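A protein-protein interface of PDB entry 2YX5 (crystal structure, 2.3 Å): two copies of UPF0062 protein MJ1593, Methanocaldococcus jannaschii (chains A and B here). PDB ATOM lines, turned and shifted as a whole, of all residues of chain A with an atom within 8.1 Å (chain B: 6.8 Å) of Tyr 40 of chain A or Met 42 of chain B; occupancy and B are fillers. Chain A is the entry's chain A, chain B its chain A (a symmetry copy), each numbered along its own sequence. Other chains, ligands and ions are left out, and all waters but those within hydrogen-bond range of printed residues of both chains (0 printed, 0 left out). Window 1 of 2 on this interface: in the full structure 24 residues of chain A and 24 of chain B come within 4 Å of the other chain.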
ATOM      1  N   THR A   5      37.770  21.818 -13.320  1.00  0.00           N
ATOM      2  CA  THR A   5      36.454  22.021 -12.767  1.00  0.00           C
ATOM      3  C   THR A   5      35.581  20.809 -13.098  1.00  0.00           C
ATOM      4  O   THR A   5      35.390  20.479 -14.270  1.00  0.00           O
ATOM      5  CB  THR A   5      35.841  23.314 -13.328  1.00  0.00           C
ATOM      6  OG1 THR A   5      36.676  24.416 -12.955  1.00  0.00           O
ATOM      7  CG2 THR A   5      34.432  23.537 -12.771  1.00  0.00           C
ATOM      8  N   VAL A   6      35.077  20.128 -12.066  1.00  0.00           N
ATOM      9  CA  VAL A   6      34.216  18.977 -12.299  1.00  0.00           C
ATOM     10  C   VAL A   6      32.771  19.292 -11.888  1.00  0.00           C
ATOM     11  O   VAL A   6      32.513  19.633 -10.738  1.00  0.00           O
ATOM     12  CB  VAL A   6      34.695  17.742 -11.511  1.00  0.00           C
ATOM     13  CG1 VAL A   6      33.881  16.505 -11.898  1.00  0.00           C
ATOM     14  CG2 VAL A   6      36.151  17.507 -11.775  1.00  0.00           C
ATOM     15  N   ILE A   7      31.846  19.217 -12.841  1.00  0.00           N
ATOM     16  CA  ILE A   7      30.436  19.433 -12.549  1.00  0.00           C
ATOM     17  C   ILE A   7      29.818  18.054 -12.548  1.00  0.00           C
ATOM     18  O   ILE A   7      30.006  17.297 -13.494  1.00  0.00           O
ATOM     19  CB  ILE A   7      29.692  20.235 -13.617  1.00  0.00           C
ATOM     20  CG1 ILE A   7      30.094  21.700 -13.580  1.00  0.00           C
ATOM     21  CG2 ILE A   7      28.221  20.117 -13.388  1.00  0.00           C
ATOM     22  CD1 ILE A   7      31.459  21.953 -14.144  1.00  0.00           C
ATOM     23  N   ILE A   8      29.106  17.725 -11.475  1.00  0.00           N
ATOM     24  CA  ILE A   8      28.453  16.435 -11.356  1.00  0.00           C
ATOM     25  C   ILE A   8      26.955  16.624 -11.138  1.00  0.00           C
ATOM     26  O   ILE A   8      26.536  17.384 -10.273  1.00  0.00           O
ATOM     27  CB  ILE A   8      28.998  15.642 -10.189  1.00  0.00           C
ATOM     28  CG1 ILE A   8      30.496  15.418 -10.378  1.00  0.00           C
ATOM     29  CG2 ILE A   8      28.252  14.321 -10.087  1.00  0.00           C
ATOM     30  CD1 ILE A   8      31.138  14.559  -9.290  1.00  0.00           C
ATOM     31  N   LYS A   9      26.158  15.927 -11.936  1.00  0.00           N
ATOM     32  CA  LYS A   9      24.710  16.012 -11.839  1.00  0.00           C
ATOM     33  C   LYS A   9      24.117  14.604 -11.907  1.00  0.00           C
ATOM     34  O   LYS A   9      24.831  13.617 -12.110  1.00  0.00           O
ATOM     35  CB  LYS A   9      24.163  16.862 -13.002  1.00  0.00           C
ATOM     36  CG  LYS A   9      24.794  16.472 -14.334  1.00  0.00           C
ATOM     37  CD  LYS A   9      24.242  17.245 -15.519  1.00  0.00           C
ATOM     38  CE  LYS A   9      24.927  16.833 -16.841  1.00  0.00           C
ATOM     39  NZ  LYS A   9      26.378  17.205 -16.925  1.00  0.00           N
ATOM     40  N   LEU A  10      22.808  14.511 -11.722  1.00  0.00           N
ATOM     41  CA  LEU A  10      22.146  13.225 -11.819  1.00  0.00           C
ATOM     42  C   LEU A  10      22.008  12.934 -13.309  1.00  0.00           C
ATOM     43  O   LEU A  10      21.994  13.861 -14.125  1.00  0.00           O
ATOM     44  CB  LEU A  10      20.762  13.281 -11.185  1.00  0.00           C
ATOM     45  CG  LEU A  10      20.688  13.385  -9.670  1.00  0.00           C
ATOM     46  CD1 LEU A  10      19.227  13.392  -9.214  1.00  0.00           C
ATOM     47  CD2 LEU A  10      21.430  12.221  -9.065  1.00  0.00           C
ATOM     48  N   ASN A  16      15.198  15.126  -9.678  1.00  0.00           N
ATOM     49  CA  ASN A  16      16.027  15.545  -8.567  1.00  0.00           C
ATOM     50  C   ASN A  16      15.212  16.244  -7.482  1.00  0.00           C
ATOM     51  O   ASN A  16      14.772  17.396  -7.629  1.00  0.00           O
ATOM     52  CB  ASN A  16      17.153  16.456  -9.085  1.00  0.00           C
ATOM     53  CG  ASN A  16      18.032  17.018  -7.970  1.00  0.00           C
ATOM     54  OD1 ASN A  16      18.186  16.421  -6.899  1.00  0.00           O
ATOM     55  ND2 ASN A  16      18.632  18.171  -8.237  1.00  0.00           N
ATOM     56  N   GLU A  18      16.068  17.642  -4.813  1.00  0.00           N
ATOM     57  CA  GLU A  18      16.595  18.925  -4.356  1.00  0.00           C
ATOM     58  C   GLU A  18      16.082  20.066  -5.254  1.00  0.00           C
ATOM     59  O   GLU A  18      15.592  21.071  -4.760  1.00  0.00           O
ATOM     60  CB  GLU A  18      18.127  18.941  -4.337  1.00  0.00           C
ATOM     61  CG  GLU A  18      18.680  20.117  -3.509  1.00  0.00           C
ATOM     62  CD  GLU A  18      20.181  20.300  -3.670  1.00  0.00           C
ATOM     63  OE1 GLU A  18      20.814  19.391  -4.264  1.00  0.00           O
ATOM     64  OE2 GLU A  18      20.730  21.338  -3.205  1.00  0.00           O
ATOM     65  N   GLY A  19      16.168  19.875  -6.565  1.00  0.00           N
ATOM     66  CA  GLY A  19      15.714  20.910  -7.468  1.00  0.00           C
ATOM     67  C   GLY A  19      14.238  21.210  -7.273  1.00  0.00           C
ATOM     68  O   GLY A  19      13.819  22.385  -7.137  1.00  0.00           O
ATOM     69  N   ILE A  22      13.569  23.093  -4.013  1.00  0.00           N
ATOM     70  CA  ILE A  22      13.936  24.480  -4.059  1.00  0.00           C
ATOM     71  C   ILE A  22      12.887  25.276  -4.825  1.00  0.00           C
ATOM     72  O   ILE A  22      12.487  26.356  -4.393  1.00  0.00           O
ATOM     73  CB  ILE A  22      15.320  24.645  -4.689  1.00  0.00           C
ATOM     74  CG1 ILE A  22      16.362  24.064  -3.725  1.00  0.00           C
ATOM     75  CG2 ILE A  22      15.585  26.106  -4.992  1.00  0.00           C
ATOM     76  CD1 ILE A  22      17.771  24.021  -4.240  1.00  0.00           C
ATOM     77  N   GLU A  36      11.715  26.854 -12.835  1.00  0.00           N
ATOM     78  CA  GLU A  36      12.397  25.582 -12.732  1.00  0.00           C
ATOM     79  C   GLU A  36      13.755  25.726 -12.058  1.00  0.00           C
ATOM     80  O   GLU A  36      14.447  26.720 -12.262  1.00  0.00           O
ATOM     81  CB  GLU A  36      12.565  25.014 -14.129  1.00  0.00           C
ATOM     82  CG  GLU A  36      13.310  23.719 -14.202  1.00  0.00           C
ATOM     83  CD  GLU A  36      13.322  23.188 -15.611  1.00  0.00           C
ATOM     84  OE1 GLU A  36      12.227  23.095 -16.205  1.00  0.00           O
ATOM     85  OE2 GLU A  36      14.412  22.868 -16.127  1.00  0.00           O
ATOM     86  N   VAL A  37      14.124  24.743 -11.237  1.00  0.00           N
ATOM     87  CA  VAL A  37      15.422  24.779 -10.565  1.00  0.00           C
ATOM     88  C   VAL A  37      16.176  23.465 -10.743  1.00  0.00           C
ATOM     89  O   VAL A  37      15.577  22.409 -10.786  1.00  0.00           O
ATOM     90  CB  VAL A  37      15.288  25.054  -9.064  1.00  0.00           C
ATOM     91  CG1 VAL A  37      16.663  24.913  -8.408  1.00  0.00           C
ATOM     92  CG2 VAL A  37      14.685  26.444  -8.829  1.00  0.00           C
ATOM     93  N   GLN A  38      17.490  23.540 -10.856  1.00  0.00           N
ATOM     94  CA  GLN A  38      18.297  22.345 -11.019  1.00  0.00           C
ATOM     95  C   GLN A  38      19.530  22.565 -10.153  1.00  0.00           C
ATOM     96  O   GLN A  38      19.938  23.705  -9.970  1.00  0.00           O
ATOM     97  CB  GLN A  38      18.697  22.149 -12.491  1.00  0.00           C
ATOM     98  CG  GLN A  38      18.317  20.770 -13.076  1.00  0.00           C
ATOM     99  CD  GLN A  38      18.962  19.563 -12.335  1.00  0.00           C
ATOM    100  OE1 GLN A  38      18.721  19.339 -11.137  1.00  0.00           O
ATOM    101  NE2 GLN A  38      19.775  18.783 -13.062  1.00  0.00           N
ATOM    102  N   THR A  39      20.100  21.493  -9.606  1.00  0.00           N
ATOM    103  CA  THR A  39      21.280  21.613  -8.759  1.00  0.00           C
ATOM    104  C   THR A  39      22.414  20.691  -9.180  1.00  0.00           C
ATOM    105  O   THR A  39      22.194  19.636  -9.759  1.00  0.00           O
ATOM    106  CB  THR A  39      20.933  21.380  -7.276  1.00  0.00           C
ATOM    107  OG1 THR A  39      20.297  20.114  -7.121  1.00  0.00           O
ATOM    108  CG2 THR A  39      19.991  22.465  -6.780  1.00  0.00           C
ATOM    109  N   TYR A  40      23.635  21.112  -8.870  1.00  0.00           N
ATOM    110  CA  TYR A  40      24.843  20.395  -9.257  1.00  0.00           C
ATOM    111  C   TYR A  40      25.883  20.529  -8.180  1.00  0.00           C
ATOM    112  O   TYR A  40      25.856  21.449  -7.368  1.00  0.00           O
ATOM    113  CB  TYR A  40      25.457  21.024 -10.510  1.00  0.00           C
ATOM    114  CG  TYR A  40      24.505  21.244 -11.635  1.00  0.00           C
ATOM    115  CD1 TYR A  40      24.197  20.206 -12.509  1.00  0.00           C
ATOM    116  CD2 TYR A  40      23.880  22.480 -11.819  1.00  0.00           C
ATOM    117  CE1 TYR A  40      23.286  20.378 -13.551  1.00  0.00           C
ATOM    118  CE2 TYR A  40      22.959  22.673 -12.862  1.00  0.00           C
ATOM    119  CZ  TYR A  40      22.665  21.611 -13.729  1.00  0.00           C
ATOM    120  OH  TYR A  40      21.755  21.746 -14.767  1.00  0.00           O
ATOM    121  N   LYS A  41      26.834  19.621  -8.201  1.00  0.00           N
ATOM    122  CA  LYS A  41      27.910  19.706  -7.252  1.00  0.00           C
ATOM    123  C   LYS A  41      29.086  20.199  -8.097  1.00  0.00           C
ATOM    124  O   LYS A  41      29.353  19.689  -9.185  1.00  0.00           O
ATOM    125  CB  LYS A  41      28.218  18.338  -6.628  1.00  0.00           C
ATOM    126  CG  LYS A  41      29.091  18.403  -5.363  1.00  0.00           C
ATOM    127  CD  LYS A  41      28.370  19.222  -4.285  1.00  0.00           C
ATOM    128  CE  LYS A  41      29.190  19.451  -3.019  1.00  0.00           C
ATOM    129  NZ  LYS A  41      28.574  20.581  -2.242  1.00  0.00           N
ATOM    130  N   MET A  42      29.755  21.226  -7.622  1.00  0.00           N
ATOM    131  CA  MET A  42      30.895  21.711  -8.344  1.00  0.00           C
ATOM    132  C   MET A  42      32.133  21.331  -7.547  1.00  0.00           C
ATOM    133  O   MET A  42      32.200  21.563  -6.353  1.00  0.00           O
ATOM    134  CB  MET A  42      30.811  23.221  -8.540  1.00  0.00           C
ATOM    135  CG  MET A  42      31.971  23.765  -9.379  1.00  0.00           C
ATOM    136  SD  MET A  42      31.718  25.421 -10.118  1.00  0.00           S
ATOM    137  CE  MET A  42      32.623  26.483  -8.912  1.00  0.00           C
ATOM    138  N   ILE A  43      33.095  20.709  -8.215  1.00  0.00           N
ATOM    139  CA  ILE A  43      34.345  20.301  -7.581  1.00  0.00           C
ATOM    140  C   ILE A  43      35.564  20.896  -8.316  1.00  0.00           C
ATOM    141  O   ILE A  43      35.854  20.519  -9.469  1.00  0.00           O
ATOM    142  CB  ILE A  43      34.485  18.762  -7.569  1.00  0.00           C
ATOM    143  CG1 ILE A  43      33.337  18.136  -6.777  1.00  0.00           C
ATOM    144  CG2 ILE A  43      35.818  18.368  -6.971  1.00  0.00           C
ATOM    145  CD1 ILE A  43      33.217  16.617  -6.923  1.00  0.00           C
ATOM    146  N   ASP A  74      26.152  11.953 -14.096  1.00  0.00           N
ATOM    147  CA  ASP A  74      26.644  12.465 -15.359  1.00  0.00           C
ATOM    148  C   ASP A  74      27.647  13.493 -14.854  1.00  0.00           C
ATOM    149  O   ASP A  74      27.477  14.023 -13.749  1.00  0.00           O
ATOM    150  CB  ASP A  74      25.538  13.150 -16.169  1.00  0.00           C
ATOM    151  CG  ASP A  74      24.833  12.195 -17.130  1.00  0.00           C
ATOM    152  OD1 ASP A  74      25.379  11.102 -17.413  1.00  0.00           O
ATOM    153  OD2 ASP A  74      23.735  12.551 -17.615  1.00  0.00           O
ATOM    154  N   GLU A  76      30.998  16.523 -16.151  1.00  0.00           N
ATOM    155  CA  GLU A  76      31.761  17.179 -17.193  1.00  0.00           C
ATOM    156  C   GLU A  76      32.979  17.856 -16.588  1.00  0.00           C
ATOM    157  O   GLU A  76      32.929  18.323 -15.454  1.00  0.00           O
ATOM    158  CB  GLU A  76      30.902  18.167 -17.978  1.00  0.00           C
ATOM    159  CG  GLU A  76      30.044  19.104 -17.170  1.00  0.00           C
ATOM    160  CD  GLU A  76      29.261  20.068 -18.066  1.00  0.00           C
ATOM    161  OE1 GLU A  76      29.913  20.875 -18.777  1.00  0.00           O
ATOM    162  OE2 GLU A  76      28.002  20.013 -18.058  1.00  0.00           O
ATOM    163  N   LYS A  78      36.252  20.692 -17.067  1.00  0.00           N
ATOM    164  CA  LYS A  78      36.874  21.850 -17.694  1.00  0.00           C
ATOM    165  C   LYS A  78      38.242  22.013 -17.031  1.00  0.00           C
ATOM    166  O   LYS A  78      38.352  21.968 -15.808  1.00  0.00           O
ATOM    167  CB  LYS A  78      36.027  23.100 -17.459  1.00  0.00           C
ATOM    168  CG  LYS A  78      34.605  22.971 -17.996  1.00  0.00           C
ATOM    169  CD  LYS A  78      33.602  23.864 -17.252  1.00  0.00           C
ATOM    170  CE  LYS A  78      32.164  23.544 -17.674  1.00  0.00           C
ATOM    171  NZ  LYS A  78      31.149  24.299 -16.890  1.00  0.00           N
ATOM    172  N   LYS B   3      18.247  32.452 -17.138  1.00  0.00           N
ATOM    173  CA  LYS B   3      18.876  31.412 -16.360  1.00  0.00           C
ATOM    174  C   LYS B   3      19.786  32.082 -15.334  1.00  0.00           C
ATOM    175  O   LYS B   3      20.787  32.700 -15.688  1.00  0.00           O
ATOM    176  CB  LYS B   3      19.696  30.486 -17.266  1.00  0.00           C
ATOM    177  CG  LYS B   3      20.586  29.498 -16.502  1.00  0.00           C
ATOM    178  CD  LYS B   3      21.385  28.584 -17.422  1.00  0.00           C
ATOM    179  CE  LYS B   3      22.445  27.842 -16.642  1.00  0.00           C
ATOM    180  NZ  LYS B   3      23.030  26.727 -17.417  1.00  0.00           N
ATOM    181  N   THR B   5      22.398  31.711 -12.319  1.00  0.00           N
ATOM    182  CA  THR B   5      23.270  30.706 -11.763  1.00  0.00           C
ATOM    183  C   THR B   5      23.717  31.149 -10.369  1.00  0.00           C
ATOM    184  O   THR B   5      24.316  32.215 -10.215  1.00  0.00           O
ATOM    185  CB  THR B   5      24.478  30.488 -12.688  1.00  0.00           C
ATOM    186  OG1 THR B   5      24.005  30.038 -13.962  1.00  0.00           O
ATOM    187  CG2 THR B   5      25.430  29.440 -12.105  1.00  0.00           C
ATOM    188  N   VAL B   6      23.400  30.346  -9.351  1.00  0.00           N
ATOM    189  CA  VAL B   6      23.812  30.686  -7.995  1.00  0.00           C
ATOM    190  C   VAL B   6      24.895  29.716  -7.502  1.00  0.00           C
ATOM    191  O   VAL B   6      24.673  28.510  -7.456  1.00  0.00           O
ATOM    192  CB  VAL B   6      22.625  30.641  -7.014  1.00  0.00           C
ATOM    193  CG1 VAL B   6      23.041  31.161  -5.636  1.00  0.00           C
ATOM    194  CG2 VAL B   6      21.490  31.457  -7.553  1.00  0.00           C
ATOM    195  N   ILE B   7      26.071  30.245  -7.176  1.00  0.00           N
ATOM    196  CA  ILE B   7      27.148  29.427  -6.636  1.00  0.00           C
ATOM    197  C   ILE B   7      27.174  29.736  -5.157  1.00  0.00           C
ATOM    198  O   ILE B   7      27.210  30.900  -4.773  1.00  0.00           O
ATOM    199  CB  ILE B   7      28.534  29.786  -7.172  1.00  0.00           C
ATOM    200  CG1 ILE B   7      28.695  29.338  -8.615  1.00  0.00           C
ATOM    201  CG2 ILE B   7      29.575  29.127  -6.328  1.00  0.00           C
ATOM    202  CD1 ILE B   7      27.946  30.196  -9.588  1.00  0.00           C
ATOM    203  N   ILE B   8      27.126  28.693  -4.334  1.00  0.00           N
ATOM    204  CA  ILE B   8      27.154  28.854  -2.892  1.00  0.00           C
ATOM    205  C   ILE B   8      28.327  28.080  -2.301  1.00  0.00           C
ATOM    206  O   ILE B   8      28.517  26.904  -2.593  1.00  0.00           O
ATOM    207  CB  ILE B   8      25.885  28.339  -2.251  1.00  0.00           C
ATOM    208  CG1 ILE B   8      24.685  29.102  -2.806  1.00  0.00           C
ATOM    209  CG2 ILE B   8      25.985  28.494  -0.742  1.00  0.00           C
ATOM    210  CD1 ILE B   8      23.352  28.713  -2.170  1.00  0.00           C
ATOM    211  N   TYR B  40      31.481  23.290  -4.152  1.00  0.00           N
ATOM    212  CA  TYR B  40      30.440  24.310  -4.183  1.00  0.00           C
ATOM    213  C   TYR B  40      29.132  23.692  -4.591  1.00  0.00           C
ATOM    214  O   TYR B  40      29.084  22.637  -5.216  1.00  0.00           O
ATOM    215  CB  TYR B  40      30.756  25.359  -5.252  1.00  0.00           C
ATOM    216  CG  TYR B  40      32.138  25.915  -5.199  1.00  0.00           C
ATOM    217  CD1 TYR B  40      32.445  26.954  -4.325  1.00  0.00           C
ATOM    218  CD2 TYR B  40      33.156  25.391  -5.999  1.00  0.00           C
ATOM    219  CE1 TYR B  40      33.738  27.471  -4.235  1.00  0.00           C
ATOM    220  CE2 TYR B  40      34.464  25.897  -5.923  1.00  0.00           C
ATOM    221  CZ  TYR B  40      34.749  26.943  -5.033  1.00  0.00           C
ATOM    222  OH  TYR B  40      36.026  27.471  -4.911  1.00  0.00           O
ATOM    223  N   LYS B  41      28.060  24.381  -4.267  1.00  0.00           N
ATOM    224  CA  LYS B  41      26.767  23.903  -4.674  1.00  0.00           C
ATOM    225  C   LYS B  41      26.386  24.847  -5.815  1.00  0.00           C
ATOM    226  O   LYS B  41      26.513  26.067  -5.709  1.00  0.00           O
ATOM    227  CB  LYS B  41      25.750  23.991  -3.527  1.00  0.00           C
ATOM    228  CG  LYS B  41      24.464  23.180  -3.761  1.00  0.00           C
ATOM    229  CD  LYS B  41      24.817  21.695  -3.919  1.00  0.00           C
ATOM    230  CE  LYS B  41      23.630  20.803  -4.268  1.00  0.00           C
ATOM    231  NZ  LYS B  41      24.147  19.495  -4.800  1.00  0.00           N
ATOM    232  N   MET B  42      25.972  24.280  -6.927  1.00  0.00           N
ATOM    233  CA  MET B  42      25.560  25.110  -8.022  1.00  0.00           C
ATOM    234  C   MET B  42      24.048  24.995  -8.134  1.00  0.00           C
ATOM    235  O   MET B  42      23.506  23.904  -8.141  1.00  0.00           O
ATOM    236  CB  MET B  42      26.240  24.678  -9.317  1.00  0.00           C
ATOM    237  CG  MET B  42      25.888  25.592 -10.493  1.00  0.00           C
ATOM    238  SD  MET B  42      27.014  25.513 -11.934  1.00  0.00           S
ATOM    239  CE  MET B  42      26.073  24.387 -13.051  1.00  0.00           C
ATOM    240  N   ILE B  43      23.372  26.135  -8.183  1.00  0.00           N
ATOM    241  CA  ILE B  43      21.919  26.175  -8.307  1.00  0.00           C
ATOM    242  C   ILE B  43      21.487  27.001  -9.537  1.00  0.00           C
ATOM    243  O   ILE B  43      21.670  28.234  -9.568  1.00  0.00           O
ATOM    244  CB  ILE B  43      21.270  26.795  -7.050  1.00  0.00           C
ATOM    245  CG1 ILE B  43      21.608  25.956  -5.817  1.00  0.00           C
ATOM    246  CG2 ILE B  43      19.772  26.889  -7.233  1.00  0.00           C
ATOM    247  CD1 ILE B  43      21.251  26.615  -4.482  1.00  0.00           C
ATOM    248  N   ASP B  44      20.924  26.311 -10.533  1.00  0.00           N
ATOM    249  CA  ASP B  44      20.435  26.949 -11.742  1.00  0.00           C
ATOM    250  C   ASP B  44      18.963  27.289 -11.646  1.00  0.00           C
ATOM    251  O   ASP B  44      18.108  26.409 -11.584  1.00  0.00           O
ATOM    252  CB  ASP B  44      20.661  26.065 -12.950  1.00  0.00           C
ATOM    253  CG  ASP B  44      22.082  26.156 -13.465  1.00  0.00           C
ATOM    254  OD1 ASP B  44      22.897  26.854 -12.818  1.00  0.00           O
ATOM    255  OD2 ASP B  44      22.381  25.532 -14.508  1.00  0.00           O
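The side-chain carboxylate (OE1) of Glu 18 of chain A is in salt-bridge range of the side-chain amino group (NZ) of Lys 41 of chain B.
N of Asp 44 of chain B sits at hydrogen-bond distance from O of Gln 38 of chain A (2.8 Å).
The backbone carbonyl oxygen (O) of Tyr 40 of chain A sits at hydrogen-bond distance from the backbone NH (N) of Met 42 of chain B (2.9 Å).
N of Met 42 of chain A lies within hydrogen-bond range of O of Tyr 40 of chain B, 2.9 Å away.
O of Lys 41 of chain A sits at hydrogen-bond distance from N of Ile 8 of chain A (3.0 Å).
The backbone NH (N) of Glu 18 of chain A lies close to the side-chain amide oxygen (OD1) of Asn 16 of chain A, 3.2 Å away.
ND2 of Asn 16 of chain A sits at hydrogen-bond distance from OG1 of Thr 39 of chain A.
The side-chain hydroxyl (OG1) of Thr 39 of chain A sits at hydrogen-bond distance from the side-chain carboxylate (OE1) of Glu 18 of chain A (3.0 Å).
NZ of Lys 3 of chain B is in salt-bridge range of OD2 of Asp 44 of chain B, 3.2 Å away.
The backbone carbonyl oxygen (O) of Ile 43 of chain B lies within hydrogen-bond range of the backbone NH (N) of Val 6 of chain B (2.7 Å).
Among the printed residues, pairs that only touch across the chains: Glu 36 of chain A with Asp 44 of chain B, Val 37 of chain A with Ile 43 of chain B, Val 37 of chain A with Asp 44 of chain B, Gln 38 of chain A with Ile 43 of chain B, Thr 39 of chain A with Met 42 of chain B, Thr 39 of chain A with Ile 43 of chain B, Tyr 40 of chain A with Lys 41 of chain B, Tyr 40 of chain A with Asp 44 of chain B and Lys 41 of chain A with Tyr 40 of chain B.
Ile 7 of chain A touches none of the printed residues of chain B.
Of the printed residues of chain B, Glu 18 of chain A touches Lys 41.
Tyr 40 of chain A touches three residues of chain B.
Ile 7 of chain B touches none of the printed residues of chain A.
Of chain A, only Glu 18 (3.1 Å) and Tyr 40 (3.6 Å) come within 4 Å of Lys 41 of chain B.
Printed residues of chain A within 4 Å of Met 42 of chain B: Thr 39 (3.3 Å) and Tyr 40 (2.9 Å).
Of the printed residues of chain A, Asp 44 of chain B touches Glu 36, Val 37, Gln 38 and Tyr 40.
The nearest printed residue of chain B that does not touch Thr 39 of chain A is Lys 41 of chain B (4.1 Å).
Of the 10 printed residues of chain B, 5 touch a printed residue of chain A.
Printed residues of chain B that touch a printed residue of chain A: Tyr 40, Lys 41, Met 42, Ile 43 and Asp 44.
Hydrophobic or aromatic side chains of chain B within 4 Å of the printed part of chain A: Tyr 40, Met 42 and Ile 43.
Hydrophobic or aromatic side chains of chain A that line the printed part of chain B: Val 37, Tyr 40 and Met 42.
Among the printed residues, 13 pairs touch across the chains.
Tyr 40 of chain A touches Lys 41 of chain B, and with the chains exchanged Lys 41 of chain A touches Tyr 40 of chain B.
Tyr 40 of chain A touches Met 42 of chain B, and with the chains exchanged Met 42 of chain A touches Tyr 40 of chain B.
Of the 13 pairs that touch across the chains among the printed residues, 4 have their exchanged pair printed and touching as well.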
